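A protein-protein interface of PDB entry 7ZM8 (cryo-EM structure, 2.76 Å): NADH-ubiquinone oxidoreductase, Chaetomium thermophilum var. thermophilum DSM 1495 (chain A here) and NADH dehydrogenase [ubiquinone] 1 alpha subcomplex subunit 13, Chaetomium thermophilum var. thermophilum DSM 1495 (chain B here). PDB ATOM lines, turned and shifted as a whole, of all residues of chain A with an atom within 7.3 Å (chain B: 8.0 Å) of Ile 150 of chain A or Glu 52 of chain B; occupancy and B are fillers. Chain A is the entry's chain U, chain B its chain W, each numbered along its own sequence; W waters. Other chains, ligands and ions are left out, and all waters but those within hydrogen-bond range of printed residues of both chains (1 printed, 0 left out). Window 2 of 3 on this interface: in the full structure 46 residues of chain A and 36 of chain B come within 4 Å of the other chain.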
ATOM      1  N   TRP A 110      -3.489  -7.613  13.827  1.00  0.00           N
ATOM      2  CA  TRP A 110      -3.443  -7.969  12.392  1.00  0.00           C
ATOM      3  C   TRP A 110      -4.766  -7.596  11.721  1.00  0.00           C
ATOM      4  O   TRP A 110      -4.779  -7.453  10.487  1.00  0.00           O
ATOM      5  CB  TRP A 110      -3.072  -9.444  12.226  1.00  0.00           C
ATOM      6  CG  TRP A 110      -3.992 -10.450  12.845  1.00  0.00           C
ATOM      7  CD1 TRP A 110      -5.065 -11.053  12.261  1.00  0.00           C
ATOM      8  CD2 TRP A 110      -3.870 -11.031  14.153  1.00  0.00           C
ATOM      9  NE1 TRP A 110      -5.636 -11.945  13.126  1.00  0.00           N
ATOM     10  CE2 TRP A 110      -4.924 -11.956  14.294  1.00  0.00           C
ATOM     11  CE3 TRP A 110      -2.987 -10.851  15.222  1.00  0.00           C
ATOM     12  CZ2 TRP A 110      -5.110 -12.700  15.455  1.00  0.00           C
ATOM     13  CZ3 TRP A 110      -3.173 -11.585  16.370  1.00  0.00           C
ATOM     14  CH2 TRP A 110      -4.223 -12.492  16.485  1.00  0.00           C
ATOM     15  N   ARG A 113      -4.660  -3.342  10.398  1.00  0.00           N
ATOM     16  CA  ARG A 113      -3.360  -2.823   9.881  1.00  0.00           C
ATOM     17  C   ARG A 113      -3.513  -1.446   9.243  1.00  0.00           C
ATOM     18  O   ARG A 113      -2.723  -0.576   9.592  1.00  0.00           O
ATOM     19  CB  ARG A 113      -2.685  -3.849   8.966  1.00  0.00           C
ATOM     20  CG  ARG A 113      -2.235  -5.112   9.677  1.00  0.00           C
ATOM     21  CD  ARG A 113      -1.205  -4.831  10.745  1.00  0.00           C
ATOM     22  NE  ARG A 113      -0.588  -6.084  11.137  1.00  0.00           N
ATOM     23  CZ  ARG A 113       0.063  -6.276  12.270  1.00  0.00           C
ATOM     24  NH1 ARG A 113       0.589  -7.458  12.530  1.00  0.00           N
ATOM     25  NH2 ARG A 113       0.188  -5.292  13.138  1.00  0.00           N
ATOM     26  N   VAL A 143       6.043  -8.900  10.273  1.00  0.00           N
ATOM     27  CA  VAL A 143       4.607  -9.265  10.124  1.00  0.00           C
ATOM     28  C   VAL A 143       3.726  -8.012  10.131  1.00  0.00           C
ATOM     29  O   VAL A 143       2.690  -8.029   9.467  1.00  0.00           O
ATOM     30  CB  VAL A 143       4.201 -10.300  11.200  1.00  0.00           C
ATOM     31  CG1 VAL A 143       3.962  -9.676  12.566  1.00  0.00           C
ATOM     32  CG2 VAL A 143       3.006 -11.137  10.771  1.00  0.00           C
ATOM     33  N   ARG A 146       3.669  -6.153   6.610  1.00  0.00           N
ATOM     34  CA  ARG A 146       3.315  -6.998   5.438  1.00  0.00           C
ATOM     35  C   ARG A 146       2.032  -6.508   4.781  1.00  0.00           C
ATOM     36  O   ARG A 146       1.070  -6.265   5.510  1.00  0.00           O
ATOM     37  CB  ARG A 146       3.085  -8.453   5.851  1.00  0.00           C
ATOM     38  CG  ARG A 146       4.351  -9.208   6.210  1.00  0.00           C
ATOM     39  CD  ARG A 146       4.163 -10.639   6.660  1.00  0.00           C
ATOM     40  NE  ARG A 146       5.476 -11.149   7.017  1.00  0.00           N
ATOM     41  CZ  ARG A 146       5.719 -12.344   7.536  1.00  0.00           C
ATOM     42  NH1 ARG A 146       6.960 -12.691   7.823  1.00  0.00           N
ATOM     43  NH2 ARG A 146       4.729 -13.185   7.764  1.00  0.00           N
ATOM     44  N   ARG A 148      -0.009  -8.265   2.986  1.00  0.00           N
ATOM     45  CA  ARG A 148      -1.075  -9.236   3.167  1.00  0.00           C
ATOM     46  C   ARG A 148      -0.999  -9.826   4.567  1.00  0.00           C
ATOM     47  O   ARG A 148       0.088 -10.164   5.045  1.00  0.00           O
ATOM     48  CB  ARG A 148      -0.983 -10.345   2.121  1.00  0.00           C
ATOM     49  CG  ARG A 148      -1.242  -9.876   0.701  1.00  0.00           C
ATOM     50  CD  ARG A 148      -1.112 -11.024  -0.281  1.00  0.00           C
ATOM     51  NE  ARG A 148      -2.163 -12.016  -0.075  1.00  0.00           N
ATOM     52  CZ  ARG A 148      -2.207 -13.199  -0.677  1.00  0.00           C
ATOM     53  NH1 ARG A 148      -3.205 -14.036  -0.427  1.00  0.00           N
ATOM     54  NH2 ARG A 148      -1.252 -13.548  -1.529  1.00  0.00           N
ATOM     55  N   GLN A 149      -2.158  -9.933   5.223  1.00  0.00           N
ATOM     56  CA  GLN A 149      -2.227 -10.625   6.531  1.00  0.00           C
ATOM     57  C   GLN A 149      -3.131 -11.830   6.324  1.00  0.00           C
ATOM     58  O   GLN A 149      -4.300 -11.633   5.990  1.00  0.00           O
ATOM     59  CB  GLN A 149      -2.795  -9.711   7.620  1.00  0.00           C
ATOM     60  CG  GLN A 149      -1.952  -8.482   7.918  1.00  0.00           C
ATOM     61  CD  GLN A 149      -0.626  -8.791   8.566  1.00  0.00           C
ATOM     62  OE1 GLN A 149      -0.484  -9.742   9.326  1.00  0.00           O
ATOM     63  NE2 GLN A 149       0.361  -7.961   8.277  1.00  0.00           N
ATOM     64  N   ILE A 150      -2.576 -13.029   6.471  1.00  0.00           N
ATOM     65  CA  ILE A 150      -3.335 -14.278   6.193  1.00  0.00           C
ATOM     66  C   ILE A 150      -4.490 -14.423   7.178  1.00  0.00           C
ATOM     67  O   ILE A 150      -5.586 -14.794   6.745  1.00  0.00           O
ATOM     68  CB  ILE A 150      -2.362 -15.472   6.290  1.00  0.00           C
ATOM     69  CG1 ILE A 150      -1.466 -15.593   5.056  1.00  0.00           C
ATOM     70  CG2 ILE A 150      -3.086 -16.774   6.588  1.00  0.00           C
ATOM     71  CD1 ILE A 150      -0.376 -16.631   5.197  1.00  0.00           C
ATOM     72  N   PHE A 151      -4.250 -14.127   8.455  1.00  0.00           N
ATOM     73  CA  PHE A 151      -5.277 -14.415   9.479  1.00  0.00           C
ATOM     74  C   PHE A 151      -6.252 -13.257   9.629  1.00  0.00           C
ATOM     75  O   PHE A 151      -7.136 -13.336  10.494  1.00  0.00           O
ATOM     76  CB  PHE A 151      -4.606 -14.925  10.752  1.00  0.00           C
ATOM     77  CG  PHE A 151      -3.812 -16.186  10.551  1.00  0.00           C
ATOM     78  CD1 PHE A 151      -4.441 -17.419  10.516  1.00  0.00           C
ATOM     79  CD2 PHE A 151      -2.439 -16.140  10.376  1.00  0.00           C
ATOM     80  CE1 PHE A 151      -3.714 -18.580  10.320  1.00  0.00           C
ATOM     81  CE2 PHE A 151      -1.714 -17.302  10.177  1.00  0.00           C
ATOM     82  CZ  PHE A 151      -2.353 -18.518  10.150  1.00  0.00           C
ATOM     83  N   ALA A 152      -6.109 -12.234   8.787  1.00  0.00           N
ATOM     84  CA  ALA A 152      -7.078 -11.108   8.803  1.00  0.00           C
ATOM     85  C   ALA A 152      -8.451 -11.552   8.300  1.00  0.00           C
ATOM     86  O   ALA A 152      -8.508 -12.217   7.263  1.00  0.00           O
ATOM     87  CB  ALA A 152      -6.568  -9.960   7.987  1.00  0.00           C
ATOM     88  N   HIS A 153      -9.510 -11.187   9.019  1.00  0.00           N
ATOM     89  CA  HIS A 153     -10.907 -11.505   8.622  1.00  0.00           C
ATOM     90  C   HIS A 153     -11.262 -10.765   7.341  1.00  0.00           C
ATOM     91  O   HIS A 153     -11.977 -11.345   6.518  1.00  0.00           O
ATOM     92  CB  HIS A 153     -11.877 -11.170   9.752  1.00  0.00           C
ATOM     93  CG  HIS A 153     -11.772 -12.067  10.937  1.00  0.00           C
ATOM     94  ND1 HIS A 153     -12.830 -12.284  11.791  1.00  0.00           N
ATOM     95  CD2 HIS A 153     -10.746 -12.802  11.412  1.00  0.00           C
ATOM     96  CE1 HIS A 153     -12.459 -13.113  12.744  1.00  0.00           C
ATOM     97  NE2 HIS A 153     -11.185 -13.441  12.535  1.00  0.00           N
ATOM     98  N   ILE A 156      -6.759  -6.710   3.255  1.00  0.00           N
ATOM     99  CA  ILE A 156      -6.161  -5.380   3.290  1.00  0.00           C
ATOM    100  C   ILE A 156      -6.134  -4.822   1.875  1.00  0.00           C
ATOM    101  O   ILE A 156      -5.585  -5.463   0.970  1.00  0.00           O
ATOM    102  CB  ILE A 156      -4.752  -5.411   3.898  1.00  0.00           C
ATOM    103  CG1 ILE A 156      -4.820  -5.781   5.378  1.00  0.00           C
ATOM    104  CG2 ILE A 156      -4.076  -4.072   3.714  1.00  0.00           C
ATOM    105  CD1 ILE A 156      -3.477  -6.000   5.999  1.00  0.00           C
ATOM    106  N   LYS B  45       1.403 -24.328   2.351  1.00  0.00           N
ATOM    107  CA  LYS B  45       0.551 -23.246   2.901  1.00  0.00           C
ATOM    108  C   LYS B  45       0.487 -23.335   4.432  1.00  0.00           C
ATOM    109  O   LYS B  45       0.292 -22.293   5.054  1.00  0.00           O
ATOM    110  CB  LYS B  45      -0.785 -23.288   2.153  1.00  0.00           C
ATOM    111  CG  LYS B  45      -0.695 -23.071   0.653  1.00  0.00           C
ATOM    112  CD  LYS B  45      -0.442 -21.636   0.278  1.00  0.00           C
ATOM    113  CE  LYS B  45      -1.621 -20.736   0.565  1.00  0.00           C
ATOM    114  NZ  LYS B  45      -1.294 -19.313   0.320  1.00  0.00           N
ATOM    115  N   LEU B  46       0.589 -24.534   5.007  1.00  0.00           N
ATOM    116  CA  LEU B  46       0.660 -24.723   6.476  1.00  0.00           C
ATOM    117  C   LEU B  46       1.987 -24.180   6.984  1.00  0.00           C
ATOM    118  O   LEU B  46       1.998 -23.596   8.062  1.00  0.00           O
ATOM    119  CB  LEU B  46       0.549 -26.210   6.808  1.00  0.00           C
ATOM    120  CG  LEU B  46       0.254 -26.524   8.271  1.00  0.00           C
ATOM    121  CD1 LEU B  46      -1.083 -25.940   8.694  1.00  0.00           C
ATOM    122  CD2 LEU B  46       0.277 -28.017   8.501  1.00  0.00           C
ATOM    123  N   VAL B  47       3.054 -24.346   6.217  1.00  0.00           N
ATOM    124  CA  VAL B  47       4.391 -23.925   6.699  1.00  0.00           C
ATOM    125  C   VAL B  47       4.367 -22.414   6.817  1.00  0.00           C
ATOM    126  O   VAL B  47       4.706 -21.894   7.878  1.00  0.00           O
ATOM    127  CB  VAL B  47       5.577 -24.459   5.866  1.00  0.00           C
ATOM    128  CG1 VAL B  47       6.852 -23.668   6.109  1.00  0.00           C
ATOM    129  CG2 VAL B  47       5.823 -25.941   6.089  1.00  0.00           C
ATOM    130  N   LYS B  48       3.905 -21.752   5.775  1.00  0.00           N
ATOM    131  CA  LYS B  48       3.879 -20.273   5.791  1.00  0.00           C
ATOM    132  C   LYS B  48       2.922 -19.731   6.855  1.00  0.00           C
ATOM    133  O   LYS B  48       3.294 -18.759   7.518  1.00  0.00           O
ATOM    134  CB  LYS B  48       3.400 -19.777   4.428  1.00  0.00           C
ATOM    135  CG  LYS B  48       4.241 -20.137   3.221  1.00  0.00           C
ATOM    136  CD  LYS B  48       3.776 -19.378   2.008  1.00  0.00           C
ATOM    137  CE  LYS B  48       3.559 -17.908   2.291  1.00  0.00           C
ATOM    138  NZ  LYS B  48       3.101 -17.178   1.086  1.00  0.00           N
ATOM    139  N   GLY B  49       1.733 -20.308   6.989  1.00  0.00           N
ATOM    140  CA  GLY B  49       0.751 -19.779   7.941  1.00  0.00           C
ATOM    141  C   GLY B  49       1.227 -19.859   9.371  1.00  0.00           C
ATOM    142  O   GLY B  49       1.064 -18.882  10.095  1.00  0.00           O
ATOM    143  N   ILE B  50       1.734 -21.014   9.795  1.00  0.00           N
ATOM    144  CA  ILE B  50       2.111 -21.154  11.229  1.00  0.00           C
ATOM    145  C   ILE B  50       3.276 -20.202  11.504  1.00  0.00           C
ATOM    146  O   ILE B  50       3.358 -19.679  12.618  1.00  0.00           O
ATOM    147  CB  ILE B  50       2.417 -22.621  11.588  1.00  0.00           C
ATOM    148  CG1 ILE B  50       1.252 -23.539  11.220  1.00  0.00           C
ATOM    149  CG2 ILE B  50       2.776 -22.745  13.057  1.00  0.00           C
ATOM    150  CD1 ILE B  50       1.476 -24.989  11.569  1.00  0.00           C
ATOM    151  N   ARG B  51       4.127 -19.973  10.509  1.00  0.00           N
ATOM    152  CA  ARG B  51       5.257 -19.020  10.662  1.00  0.00           C
ATOM    153  C   ARG B  51       4.708 -17.603  10.880  1.00  0.00           C
ATOM    154  O   ARG B  51       5.290 -16.873  11.690  1.00  0.00           O
ATOM    155  CB  ARG B  51       6.242 -19.213   9.508  1.00  0.00           C
ATOM    156  CG  ARG B  51       7.206 -20.368   9.722  1.00  0.00           C
ATOM    157  CD  ARG B  51       8.176 -20.551   8.573  1.00  0.00           C
ATOM    158  NE  ARG B  51       9.150 -21.594   8.854  1.00  0.00           N
ATOM    159  CZ  ARG B  51      10.032 -22.047   7.973  1.00  0.00           C
ATOM    160  NH1 ARG B  51      10.883 -22.997   8.316  1.00  0.00           N
ATOM    161  NH2 ARG B  51      10.057 -21.552   6.750  1.00  0.00           N
ATOM    162  N   GLU B  52       3.618 -17.239  10.198  1.00  0.00           N
ATOM    163  CA  GLU B  52       2.968 -15.916  10.394  1.00  0.00           C
ATOM    164  C   GLU B  52       2.301 -15.862  11.774  1.00  0.00           C
ATOM    165  O   GLU B  52       2.427 -14.822  12.430  1.00  0.00           O
ATOM    166  CB  GLU B  52       1.966 -15.662   9.267  1.00  0.00           C
ATOM    167  CG  GLU B  52       1.241 -14.336   9.359  1.00  0.00           C
ATOM    168  CD  GLU B  52       0.927 -13.707   8.010  1.00  0.00           C
ATOM    169  OE1 GLU B  52       1.665 -13.984   7.043  1.00  0.00           O
ATOM    170  OE2 GLU B  52      -0.052 -12.944   7.930  1.00  0.00           O
ATOM    171  N   GLN B  53       1.634 -16.935  12.196  1.00  0.00           N
ATOM    172  CA  GLN B  53       0.951 -16.984  13.507  1.00  0.00           C
ATOM    173  C   GLN B  53       1.983 -16.778  14.601  1.00  0.00           C
ATOM    174  O   GLN B  53       1.664 -16.132  15.591  1.00  0.00           O
ATOM    175  CB  GLN B  53       0.363 -18.367  13.752  1.00  0.00           C
ATOM    176  CG  GLN B  53      -1.145 -18.454  13.630  1.00  0.00           C
ATOM    177  CD  GLN B  53      -1.568 -19.895  13.751  1.00  0.00           C
ATOM    178  OE1 GLN B  53      -0.774 -20.759  14.106  1.00  0.00           O
ATOM    179  NE2 GLN B  53      -2.825 -20.166  13.455  1.00  0.00           N
ATOM    180  N   ASN B  54       3.172 -17.332  14.430  1.00  0.00           N
ATOM    181  CA  ASN B  54       4.200 -17.295  15.493  1.00  0.00           C
ATOM    182  C   ASN B  54       4.821 -15.909  15.564  1.00  0.00           C
ATOM    183  O   ASN B  54       5.363 -15.574  16.612  1.00  0.00           O
ATOM    184  CB  ASN B  54       5.196 -18.431  15.297  1.00  0.00           C
ATOM    185  CG  ASN B  54       4.658 -19.796  15.656  1.00  0.00           C
ATOM    186  OD1 ASN B  54       3.511 -19.934  16.061  1.00  0.00           O
ATOM    187  ND2 ASN B  54       5.482 -20.817  15.511  1.00  0.00           N
ATOM    188  N   GLU B  55       4.723 -15.145  14.485  1.00  0.00           N
ATOM    189  CA  GLU B  55       5.244 -13.761  14.456  1.00  0.00           C
ATOM    190  C   GLU B  55       4.146 -12.799  14.921  1.00  0.00           C
ATOM    191  O   GLU B  55       4.471 -11.735  15.445  1.00  0.00           O
ATOM    192  CB  GLU B  55       5.852 -13.515  13.074  1.00  0.00           C
ATOM    193  CG  GLU B  55       7.125 -14.301  12.842  1.00  0.00           C
ATOM    194  CD  GLU B  55       8.094 -14.280  14.011  1.00  0.00           C
ATOM    195  OE1 GLU B  55       8.610 -15.359  14.369  1.00  0.00           O
ATOM    196  OE2 GLU B  55       8.345 -13.183  14.550  1.00  0.00           O
ATOM    197  N   LEU B  56       2.889 -13.157  14.733  1.00  0.00           N
ATOM    198  CA  LEU B  56       1.760 -12.391  15.310  1.00  0.00           C
ATOM    199  C   LEU B  56       1.774 -12.550  16.821  1.00  0.00           C
ATOM    200  O   LEU B  56       1.458 -11.592  17.516  1.00  0.00           O
ATOM    201  CB  LEU B  56       0.458 -12.894  14.685  1.00  0.00           C
ATOM    202  CG  LEU B  56       0.209 -12.483  13.240  1.00  0.00           C
ATOM    203  CD1 LEU B  56      -1.034 -13.170  12.710  1.00  0.00           C
ATOM    204  CD2 LEU B  56       0.091 -10.977  13.122  1.00  0.00           C
ATOM    205  N   ALA B  57       2.112 -13.736  17.298  1.00  0.00           N
ATOM    206  CA  ALA B  57       2.221 -14.009  18.742  1.00  0.00           C
ATOM    207  C   ALA B  57       3.366 -13.193  19.353  1.00  0.00           C
ATOM    208  O   ALA B  57       3.209 -12.742  20.492  1.00  0.00           O
ATOM    209  CB  ALA B  57       2.347 -15.489  18.981  1.00  0.00           C
ATOM    210  N   ARG B  58       4.469 -13.022  18.636  1.00  0.00           N
ATOM    211  CA  ARG B  58       5.611 -12.222  19.126  1.00  0.00           C
ATOM    212  C   ARG B  58       5.163 -10.778  19.324  1.00  0.00           C
ATOM    213  O   ARG B  58       5.580 -10.180  20.314  1.00  0.00           O
ATOM    214  CB  ARG B  58       6.771 -12.261  18.133  1.00  0.00           C
ATOM    215  CG  ARG B  58       8.055 -11.643  18.664  1.00  0.00           C
ATOM    216  CD  ARG B  58       9.192 -11.703  17.667  1.00  0.00           C
ATOM    217  NE  ARG B  58       9.420 -13.059  17.200  1.00  0.00           N
ATOM    218  CZ  ARG B  58      10.214 -13.936  17.797  1.00  0.00           C
ATOM    219  NH1 ARG B  58      10.352 -15.149  17.293  1.00  0.00           N
ATOM    220  NH2 ARG B  58      10.864 -13.602  18.893  1.00  0.00           N
ATOM    221  N   GLU B  59       4.297 -10.257  18.463  1.00  0.00           N
ATOM    222  CA  GLU B  59       3.914  -8.834  18.544  1.00  0.00           C
ATOM    223  C   GLU B  59       2.865  -8.684  19.636  1.00  0.00           C
ATOM    224  O   GLU B  59       2.867  -7.661  20.313  1.00  0.00           O
ATOM    225  CB  GLU B  59       3.244  -8.455  17.232  1.00  0.00           C
ATOM    226  CG  GLU B  59       2.701  -7.044  17.187  1.00  0.00           C
ATOM    227  CD  GLU B  59       1.980  -6.718  15.895  1.00  0.00           C
ATOM    228  OE1 GLU B  59       1.701  -7.657  15.131  1.00  0.00           O
ATOM    229  OE2 GLU B  59       1.706  -5.530  15.655  1.00  0.00           O
HETATM  230  O   HOH W   1      -1.998 -12.282   9.777  1.00  0.00           O
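The side-chain carboxylate (OE1) of Glu 59 of chain B lies within salt-bridge range of the guanidinium group (NH1) of Arg 113 of chain A, 2.8 Å away. The guanidinium group (NH2) of Arg 146 of chain A lies within salt-bridge range of the side-chain carboxylate (OE1) of Glu 52 of chain B, at 3.2 Å. The backbone NH of Ile 150 of chain A is in hydrogen-bond range of the side-chain carboxylate of Glu 52 of chain B (2.9 Å).
Among the printed residues, merely in contact across the chains: Phe 151 of chain A with Gly 49 of chain B, Gln 149 of chain A with Glu 52 of chain B, Val 143 of chain A with Glu 55 of chain B, Arg 113 of chain A with Leu 56 of chain B, Phe 151 of chain A with Gln 53 of chain B, Trp 110 of chain A with Leu 56 of chain B, Val 143 of chain A with Leu 56 of chain B, Val 143 of chain A with Glu 52 of chain B and Val 143 of chain A with Glu 59 of chain B.
Printed residues of chain A that touch a printed residue of chain B: Trp 110, Arg 113, Val 143, Arg 146, Gln 149, Ile 150 and Phe 151. Hydrophobic or aromatic side chains of chain A within 4 Å of the printed part of chain B: Trp 110, Val 143, Ile 150 and Phe 151. Of the 15 printed residues of chain B, 6 touch a printed residue of chain A. Along chain B the printed residues that touch a printed residue of chain A span positions 49 to 59. Among the printed residues, 12 pairs touch across the chains.
Of the printed residues of chain B, Trp 110 of chain A touches Leu 56. Of chain B, only Glu 52 (2.9 Å) comes within 4 Å of Ile 150 of chain A. Of the printed residues of chain B, Phe 151 of chain A touches Gly 49 and Gln 53. Printed residues of chain A within 4 Å of Gly 49 of chain B: Phe 151 (3.2 Å). The nearest printed residue of chain A that does not touch Glu 52 of chain B is Arg 148 of chain A (4.01 Å).
The indole nitrogen (NE1) of Trp 110 of chain A lies within hydrogen-bond range of the backbone carbonyl oxygen (O) of Phe 151 of chain A (3.3 Å). The side-chain amide nitrogen (NE2) of Gln 149 of chain A lies within hydrogen-bond range of the backbone carbonyl oxygen (O) of Val 143 of chain A (2.6 Å). NE2 of Gln 149 of chain A lies within hydrogen-bond range of O of Arg 146 of chain A (3.3 Å). OE2 of Glu 55 of chain B lies within salt-bridge range of NE of Arg 58 of chain B, 2.9 Å away.
Water W1 lies within hydrogen-bond range of OE2 of Glu 52 of chain B, OE1 of Gln 149 of chain A, N of Phe 151 of chain A and N of Ile 150 of chain A.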
